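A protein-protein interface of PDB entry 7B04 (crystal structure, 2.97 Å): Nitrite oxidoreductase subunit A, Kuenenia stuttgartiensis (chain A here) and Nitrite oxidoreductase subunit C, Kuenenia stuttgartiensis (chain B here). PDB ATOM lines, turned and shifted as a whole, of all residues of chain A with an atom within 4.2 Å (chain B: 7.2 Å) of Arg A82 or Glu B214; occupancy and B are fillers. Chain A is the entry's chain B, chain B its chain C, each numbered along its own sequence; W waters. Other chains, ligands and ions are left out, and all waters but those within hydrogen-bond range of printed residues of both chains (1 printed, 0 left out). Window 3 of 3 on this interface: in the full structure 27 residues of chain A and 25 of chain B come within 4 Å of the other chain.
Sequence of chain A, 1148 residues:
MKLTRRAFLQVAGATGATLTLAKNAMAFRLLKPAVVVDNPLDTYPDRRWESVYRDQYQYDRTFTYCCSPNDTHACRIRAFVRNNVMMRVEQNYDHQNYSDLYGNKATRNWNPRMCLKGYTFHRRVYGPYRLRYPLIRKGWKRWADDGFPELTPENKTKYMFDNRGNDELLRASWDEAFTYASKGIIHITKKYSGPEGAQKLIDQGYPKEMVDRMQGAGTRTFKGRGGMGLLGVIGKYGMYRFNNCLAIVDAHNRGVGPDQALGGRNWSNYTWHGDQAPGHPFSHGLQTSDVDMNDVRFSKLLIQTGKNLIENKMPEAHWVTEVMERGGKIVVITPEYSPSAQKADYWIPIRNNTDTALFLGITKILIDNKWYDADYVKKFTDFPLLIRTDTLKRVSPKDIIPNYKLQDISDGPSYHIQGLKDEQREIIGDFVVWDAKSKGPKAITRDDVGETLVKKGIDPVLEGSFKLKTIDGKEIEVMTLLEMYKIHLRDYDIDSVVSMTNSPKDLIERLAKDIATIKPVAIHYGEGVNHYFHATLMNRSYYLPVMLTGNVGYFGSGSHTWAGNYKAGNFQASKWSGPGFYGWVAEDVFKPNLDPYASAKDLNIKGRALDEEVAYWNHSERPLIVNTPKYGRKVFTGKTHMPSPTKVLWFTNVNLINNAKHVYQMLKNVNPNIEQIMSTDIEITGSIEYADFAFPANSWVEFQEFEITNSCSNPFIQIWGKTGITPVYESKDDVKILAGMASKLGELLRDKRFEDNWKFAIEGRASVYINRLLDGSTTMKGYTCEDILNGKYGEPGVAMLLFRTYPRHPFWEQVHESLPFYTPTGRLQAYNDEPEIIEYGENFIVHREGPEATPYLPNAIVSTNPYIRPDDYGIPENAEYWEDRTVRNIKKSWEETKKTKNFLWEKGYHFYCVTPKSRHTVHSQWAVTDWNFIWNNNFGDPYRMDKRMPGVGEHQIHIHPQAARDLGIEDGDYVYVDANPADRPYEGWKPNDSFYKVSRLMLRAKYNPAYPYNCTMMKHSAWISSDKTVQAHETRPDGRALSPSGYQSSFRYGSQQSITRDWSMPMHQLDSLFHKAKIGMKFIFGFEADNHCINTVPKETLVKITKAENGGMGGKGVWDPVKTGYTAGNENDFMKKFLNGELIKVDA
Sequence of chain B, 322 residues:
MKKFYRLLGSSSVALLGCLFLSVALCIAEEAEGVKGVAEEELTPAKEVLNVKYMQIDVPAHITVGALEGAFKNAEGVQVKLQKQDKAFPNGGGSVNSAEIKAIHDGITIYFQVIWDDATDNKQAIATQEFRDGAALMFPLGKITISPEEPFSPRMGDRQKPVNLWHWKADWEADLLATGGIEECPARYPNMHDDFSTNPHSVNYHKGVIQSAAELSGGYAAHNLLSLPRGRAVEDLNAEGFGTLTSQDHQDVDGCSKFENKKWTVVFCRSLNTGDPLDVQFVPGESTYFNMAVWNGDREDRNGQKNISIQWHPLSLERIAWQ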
ATOM      1  N   ASP A  55     -14.574   0.444 -33.111  1.00  0.00           N
ATOM      2  CA  ASP A  55     -14.224   1.210 -31.894  1.00  0.00           C
ATOM      3  C   ASP A  55     -15.494   1.628 -31.165  1.00  0.00           C
ATOM      4  O   ASP A  55     -15.465   1.739 -29.974  1.00  0.00           O
ATOM      5  CB  ASP A  55     -13.477   2.475 -32.259  1.00  0.00           C
ATOM      6  CG  ASP A  55     -12.093   2.223 -32.786  1.00  0.00           C
ATOM      7  OD1 ASP A  55     -11.641   1.111 -32.635  1.00  0.00           O
ATOM      8  OD2 ASP A  55     -11.493   3.156 -33.312  1.00  0.00           O
ATOM      9  N   GLN A  56     -16.527   2.000 -31.903  1.00  0.00           N
ATOM     10  CA  GLN A  56     -17.805   2.428 -31.300  1.00  0.00           C
ATOM     11  C   GLN A  56     -18.482   1.261 -30.584  1.00  0.00           C
ATOM     12  O   GLN A  56     -19.037   1.482 -29.530  1.00  0.00           O
ATOM     13  CB  GLN A  56     -18.710   3.017 -32.378  1.00  0.00           C
ATOM     14  CG  GLN A  56     -19.580   4.163 -31.903  1.00  0.00           C
ATOM     15  CD  GLN A  56     -20.647   4.526 -32.892  1.00  0.00           C
ATOM     16  OE1 GLN A  56     -20.671   4.040 -33.987  1.00  0.00           O
ATOM     17  NE2 GLN A  56     -21.522   5.421 -32.531  1.00  0.00           N
ATOM     18  N   GLN A  58     -17.230  -1.320 -29.072  1.00  0.00           N
ATOM     19  CA  GLN A  58     -16.415  -1.820 -27.939  1.00  0.00           C
ATOM     20  C   GLN A  58     -16.984  -1.487 -26.566  1.00  0.00           C
ATOM     21  O   GLN A  58     -17.358  -0.380 -26.365  1.00  0.00           O
ATOM     22  CB  GLN A  58     -15.126  -1.023 -27.985  1.00  0.00           C
ATOM     23  CG  GLN A  58     -13.877  -1.839 -27.822  1.00  0.00           C
ATOM     24  CD  GLN A  58     -12.901  -0.965 -27.104  1.00  0.00           C
ATOM     25  OE1 GLN A  58     -12.267  -0.101 -27.692  1.00  0.00           O
ATOM     26  NE2 GLN A  58     -12.824  -1.153 -25.808  1.00  0.00           N
ATOM     27  N   ASP A  60     -16.403  -2.632 -22.094  1.00  0.00           N
ATOM     28  CA  ASP A  60     -15.437  -3.207 -21.159  1.00  0.00           C
ATOM     29  C   ASP A  60     -16.004  -4.341 -20.320  1.00  0.00           C
ATOM     30  O   ASP A  60     -15.346  -5.369 -20.132  1.00  0.00           O
ATOM     31  CB  ASP A  60     -14.912  -2.133 -20.203  1.00  0.00           C
ATOM     32  CG  ASP A  60     -14.591  -0.830 -20.896  1.00  0.00           C
ATOM     33  OD1 ASP A  60     -15.300   0.155 -20.654  1.00  0.00           O
ATOM     34  OD2 ASP A  60     -13.620  -0.784 -21.672  1.00  0.00           O
ATOM     35  N   VAL A  81     -21.411  -2.055 -20.739  1.00  0.00           N
ATOM     36  CA  VAL A  81     -20.832  -0.866 -20.126  1.00  0.00           C
ATOM     37  C   VAL A  81     -19.522  -0.534 -20.827  1.00  0.00           C
ATOM     38  O   VAL A  81     -18.741  -1.430 -21.166  1.00  0.00           O
ATOM     39  CB  VAL A  81     -20.616  -1.080 -18.615  1.00  0.00           C
ATOM     40  CG1 VAL A  81     -19.839   0.067 -18.009  1.00  0.00           C
ATOM     41  CG2 VAL A  81     -21.949  -1.235 -17.912  1.00  0.00           C
ATOM     42  N   ARG A  82     -19.292   0.748 -21.062  1.00  0.00           N
ATOM     43  CA  ARG A  82     -18.006   1.200 -21.630  1.00  0.00           C
ATOM     44  C   ARG A  82     -17.499   2.292 -20.706  1.00  0.00           C
ATOM     45  O   ARG A  82     -18.182   3.280 -20.587  1.00  0.00           O
ATOM     46  CB  ARG A  82     -18.217   1.803 -23.010  1.00  0.00           C
ATOM     47  CG  ARG A  82     -16.963   2.444 -23.561  1.00  0.00           C
ATOM     48  CD  ARG A  82     -17.268   3.233 -24.793  1.00  0.00           C
ATOM     49  NE  ARG A  82     -16.521   2.711 -25.908  1.00  0.00           N
ATOM     50  CZ  ARG A  82     -15.528   3.343 -26.465  1.00  0.00           C
ATOM     51  NH1 ARG A  82     -15.300   4.600 -26.157  1.00  0.00           N
ATOM     52  NH2 ARG A  82     -14.756   2.716 -27.313  1.00  0.00           N
ATOM     53  N   ASN A  83     -16.339   2.083 -20.106  1.00  0.00           N
ATOM     54  CA  ASN A  83     -15.698   2.992 -19.155  1.00  0.00           C
ATOM     55  C   ASN A  83     -16.677   3.410 -18.058  1.00  0.00           C
ATOM     56  O   ASN A  83     -16.864   4.593 -17.767  1.00  0.00           O
ATOM     57  CB  ASN A  83     -15.104   4.209 -19.867  1.00  0.00           C
ATOM     58  CG  ASN A  83     -13.955   4.831 -19.094  1.00  0.00           C
ATOM     59  OD1 ASN A  83     -13.620   4.392 -17.993  1.00  0.00           O
ATOM     60  ND2 ASN A  83     -13.343   5.859 -19.671  1.00  0.00           N
ATOM     61  N   ASN A  84     -17.308   2.404 -17.447  1.00  0.00           N
ATOM     62  CA  ASN A  84     -18.227   2.585 -16.321  1.00  0.00           C
ATOM     63  C   ASN A  84     -19.426   3.465 -16.675  1.00  0.00           C
ATOM     64  O   ASN A  84     -19.984   4.153 -15.815  1.00  0.00           O
ATOM     65  CB  ASN A  84     -17.497   3.112 -15.084  1.00  0.00           C
ATOM     66  CG  ASN A  84     -16.812   2.000 -14.312  1.00  0.00           C
ATOM     67  OD1 ASN A  84     -17.470   1.158 -13.699  1.00  0.00           O
ATOM     68  ND2 ASN A  84     -15.485   1.979 -14.354  1.00  0.00           N
ATOM     69  N   VAL A  85     -19.823   3.463 -17.945  1.00  0.00           N
ATOM     70  CA  VAL A  85     -21.032   4.135 -18.407  1.00  0.00           C
ATOM     71  C   VAL A  85     -21.900   3.091 -19.094  1.00  0.00           C
ATOM     72  O   VAL A  85     -21.430   2.383 -19.992  1.00  0.00           O
ATOM     73  CB  VAL A  85     -20.719   5.306 -19.357  1.00  0.00           C
ATOM     74  CG1 VAL A  85     -22.006   5.949 -19.850  1.00  0.00           C
ATOM     75  CG2 VAL A  85     -19.842   6.333 -18.664  1.00  0.00           C
ATOM     76  N   MET A  87     -24.021   1.837 -21.703  1.00  0.00           N
ATOM     77  CA  MET A  87     -24.156   2.298 -23.100  1.00  0.00           C
ATOM     78  C   MET A  87     -25.360   1.721 -23.821  1.00  0.00           C
ATOM     79  O   MET A  87     -26.045   2.451 -24.476  1.00  0.00           O
ATOM     80  CB  MET A  87     -22.895   1.907 -23.858  1.00  0.00           C
ATOM     81  CG  MET A  87     -21.684   2.448 -23.219  1.00  0.00           C
ATOM     82  SD  MET A  87     -21.429   4.119 -23.662  1.00  0.00           S
ATOM     83  CE  MET A  87     -21.940   4.083 -25.370  1.00  0.00           C
ATOM     84  N   TYR B 204     -18.866  12.325 -16.519  1.00  0.00           N
ATOM     85  CA  TYR B 204     -18.358  11.128 -17.182  1.00  0.00           C
ATOM     86  C   TYR B 204     -19.308  10.585 -18.239  1.00  0.00           C
ATOM     87  O   TYR B 204     -18.864   9.899 -19.167  1.00  0.00           O
ATOM     88  CB  TYR B 204     -18.053  10.040 -16.154  1.00  0.00           C
ATOM     89  CG  TYR B 204     -19.211   9.655 -15.271  1.00  0.00           C
ATOM     90  CD1 TYR B 204     -19.300  10.117 -13.966  1.00  0.00           C
ATOM     91  CD2 TYR B 204     -20.210   8.817 -15.737  1.00  0.00           C
ATOM     92  CE1 TYR B 204     -20.357   9.749 -13.156  1.00  0.00           C
ATOM     93  CE2 TYR B 204     -21.273   8.452 -14.935  1.00  0.00           C
ATOM     94  CZ  TYR B 204     -21.343   8.920 -13.646  1.00  0.00           C
ATOM     95  OH  TYR B 204     -22.396   8.557 -12.836  1.00  0.00           O
ATOM     96  N   GLY B 207     -18.776  12.811 -21.281  1.00  0.00           N
ATOM     97  CA  GLY B 207     -17.427  12.571 -21.762  1.00  0.00           C
ATOM     98  C   GLY B 207     -17.317  11.325 -22.618  1.00  0.00           C
ATOM     99  O   GLY B 207     -16.614  11.320 -23.630  1.00  0.00           O
ATOM    100  N   VAL B 208     -18.004  10.255 -22.224  1.00  0.00           N
ATOM    101  CA  VAL B 208     -17.991   9.024 -23.006  1.00  0.00           C
ATOM    102  C   VAL B 208     -18.860   9.160 -24.251  1.00  0.00           C
ATOM    103  O   VAL B 208     -18.451   8.789 -25.358  1.00  0.00           O
ATOM    104  CB  VAL B 208     -18.427   7.831 -22.136  1.00  0.00           C
ATOM    105  CG1 VAL B 208     -18.647   6.595 -22.994  1.00  0.00           C
ATOM    106  CG2 VAL B 208     -17.385   7.558 -21.065  1.00  0.00           C
ATOM    107  N   ILE B 209     -20.073   9.695 -24.092  1.00  0.00           N
ATOM    108  CA  ILE B 209     -21.029   9.715 -25.197  1.00  0.00           C
ATOM    109  C   ILE B 209     -20.542  10.623 -26.319  1.00  0.00           C
ATOM    110  O   ILE B 209     -20.635  10.274 -27.502  1.00  0.00           O
ATOM    111  CB  ILE B 209     -22.421  10.138 -24.692  1.00  0.00           C
ATOM    112  CG1 ILE B 209     -22.975   9.094 -23.721  1.00  0.00           C
ATOM    113  CG2 ILE B 209     -23.373  10.341 -25.860  1.00  0.00           C
ATOM    114  CD1 ILE B 209     -23.139   7.720 -24.329  1.00  0.00           C
ATOM    115  N   GLN B 210     -20.010  11.795 -25.974  1.00  0.00           N
ATOM    116  CA  GLN B 210     -19.503  12.730 -26.968  1.00  0.00           C
ATOM    117  C   GLN B 210     -17.992  12.631 -27.145  1.00  0.00           C
ATOM    118  O   GLN B 210     -17.362  13.589 -27.604  1.00  0.00           O
ATOM    119  CB  GLN B 210     -19.916  14.159 -26.612  1.00  0.00           C
ATOM    120  CG  GLN B 210     -21.422  14.375 -26.670  1.00  0.00           C
ATOM    121  CD  GLN B 210     -21.816  15.834 -26.564  1.00  0.00           C
ATOM    122  OE1 GLN B 210     -20.962  16.719 -26.518  1.00  0.00           O
ATOM    123  NE2 GLN B 210     -23.119  16.092 -26.526  1.00  0.00           N
ATOM    124  N   SER B 211     -17.401  11.494 -26.787  1.00  0.00           N
ATOM    125  CA  SER B 211     -16.020  11.219 -27.148  1.00  0.00           C
ATOM    126  C   SER B 211     -15.911  10.982 -28.651  1.00  0.00           C
ATOM    127  O   SER B 211     -16.888  10.642 -29.326  1.00  0.00           O
ATOM    128  CB  SER B 211     -15.489  10.012 -26.375  1.00  0.00           C
ATOM    129  OG  SER B 211     -16.191   8.832 -26.722  1.00  0.00           O
ATOM    130  N   ALA B 212     -14.697  11.170 -29.176  1.00  0.00           N
ATOM    131  CA  ALA B 212     -14.484  11.040 -30.615  1.00  0.00           C
ATOM    132  C   ALA B 212     -14.865   9.650 -31.117  1.00  0.00           C
ATOM    133  O   ALA B 212     -15.489   9.518 -32.175  1.00  0.00           O
ATOM    134  CB  ALA B 212     -13.028  11.356 -30.959  1.00  0.00           C
ATOM    135  N   ALA B 213     -14.580   8.627 -30.343  1.00  0.00           N
ATOM    136  CA  ALA B 213     -14.939   7.256 -30.735  1.00  0.00           C
ATOM    137  C   ALA B 213     -16.446   7.099 -30.804  1.00  0.00           C
ATOM    138  O   ALA B 213     -16.921   6.431 -31.672  1.00  0.00           O
ATOM    139  CB  ALA B 213     -14.389   6.309 -29.716  1.00  0.00           C
ATOM    140  N   GLU B 214     -17.160   7.672 -29.857  1.00  0.00           N
ATOM    141  CA  GLU B 214     -18.621   7.481 -29.818  1.00  0.00           C
ATOM    142  C   GLU B 214     -19.309   8.466 -30.739  1.00  0.00           C
ATOM    143  O   GLU B 214     -20.459   8.248 -31.050  1.00  0.00           O
ATOM    144  CB  GLU B 214     -19.103   7.545 -28.386  1.00  0.00           C
ATOM    145  CG  GLU B 214     -18.564   6.401 -27.592  1.00  0.00           C
ATOM    146  CD  GLU B 214     -19.171   5.109 -28.041  1.00  0.00           C
ATOM    147  OE1 GLU B 214     -20.328   5.088 -28.250  1.00  0.00           O
ATOM    148  OE2 GLU B 214     -18.474   4.168 -28.186  1.00  0.00           O
ATOM    149  N   LEU B 215     -18.621   9.520 -31.136  1.00  0.00           N
ATOM    150  CA  LEU B 215     -19.297  10.432 -32.075  1.00  0.00           C
ATOM    151  C   LEU B 215     -19.441   9.700 -33.410  1.00  0.00           C
ATOM    152  O   LEU B 215     -20.520   9.745 -33.973  1.00  0.00           O
ATOM    153  CB  LEU B 215     -18.469  11.708 -32.167  1.00  0.00           C
ATOM    154  CG  LEU B 215     -18.790  12.760 -31.114  1.00  0.00           C
ATOM    155  CD1 LEU B 215     -17.740  13.834 -31.069  1.00  0.00           C
ATOM    156  CD2 LEU B 215     -20.141  13.378 -31.368  1.00  0.00           C
ATOM    157  N   SER B 216     -18.369   9.030 -33.830  1.00  0.00           N
ATOM    158  CA  SER B 216     -18.191   8.162 -35.025  1.00  0.00           C
ATOM    159  C   SER B 216     -18.110   8.956 -36.323  1.00  0.00           C
ATOM    160  O   SER B 216     -17.813  10.119 -36.272  1.00  0.00           O
ATOM    161  CB  SER B 216     -19.202   7.079 -35.105  1.00  0.00           C
ATOM    162  OG  SER B 216     -18.628   5.884 -35.542  1.00  0.00           O
ATOM    163  N   GLY B 217     -18.281   8.265 -37.438  1.00  0.00           N
ATOM    164  CA  GLY B 217     -18.333   8.839 -38.787  1.00  0.00           C
ATOM    165  C   GLY B 217     -17.131   9.668 -39.139  1.00  0.00           C
ATOM    166  O   GLY B 217     -16.043   9.269 -38.813  1.00  0.00           O
ATOM    167  N   ALA B 220     -14.901  10.653 -36.059  1.00  0.00           N
ATOM    168  CA  ALA B 220     -13.946   9.655 -35.590  1.00  0.00           C
ATOM    169  C   ALA B 220     -12.883   9.344 -36.637  1.00  0.00           C
ATOM    170  O   ALA B 220     -11.738   9.047 -36.281  1.00  0.00           O
ATOM    171  CB  ALA B 220     -14.675   8.369 -35.188  1.00  0.00           C
HETATM  172  O   HOH W   1     -21.989   2.421 -29.515  1.00  0.00           O
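The side-chain hydroxyl (OG) of Ser B211 lies within hydrogen-bond range of the backbone carbonyl oxygen (O) of Val B208. The side-chain hydroxyl of Ser B211 lies within hydrogen-bond range of the backbone NH of Glu B214, at 3.5 Å. O of Gln A58 sits at hydrogen-bond distance from NE of Arg A82, 3.2 Å away. The backbone carbonyl oxygen (O) of Asp A55 is in hydrogen-bond range of the guanidinium group (NH2) of Arg A82, 2.9 Å away.
Of chain B, only Glu B214 (3.3 Å) comes within 4 Å of Arg A82. Printed residues of chain B within 4 Å of Met A87: Val B208 (3.8 Å), Ile B209 (3.97 Å) and Glu B214 (3.5 Å). Printed residues of chain A within 4 Å of Val B208: Val A85 and Met A87. Of the printed residues of chain A, Ser B216 touches Gln A56. The nearest printed residue of chain B that does not touch Arg A82 is Ala B213 (4.1 Å). The nearest printed residue of chain A that does not touch Tyr B204 is Asn A84 (4.6 Å).
The side-chain hydroxyl (OG) of Ser B216 is in hydrogen-bond range of the side-chain amide oxygen (OE1) of Gln A56 (3.2 Å). The backbone carbonyl oxygen of Glu B214 sits at hydrogen-bond distance from the side-chain amide nitrogen of Gln A56, at 3.4 Å. The side-chain carboxylate (OE2) of Glu B214 is in salt-bridge range of the guanidinium group (NE) of Arg A82 (3.3 Å).
Among the printed residues, merely in contact across the chains: Gln A56 with Ala B213 (3.5 Å), Val A85 with Tyr B204 (3.7 Å), Val A85 with Val B208 (3.6 Å), Met A87 with Val B208 (3.8 Å), Met A87 with Ile B209 (3.97 Å) and Met A87 with Glu B214 (3.5 Å).
Water W1 lies within hydrogen-bond range of O of Gln A56 and OE1 of Glu B214.
Hydrophobic or aromatic side chains of chain A within 4 Å of the printed part of chain B: Val A85 and Met A87. Along chain A the printed residues that touch a printed residue of chain B span positions 56 to 87. Of the 13 printed residues of chain B, 6 touch a printed residue of chain A. Hydrophobic or aromatic side chains of chain B that line the printed part of chain A: Tyr B204, Val B208 and Ile B209. Among the printed residues, Asp or Glu carboxylates within 4 Å of a Lys or Arg side-chain nitrogen of the other chain: Arg A82 with Glu B214.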
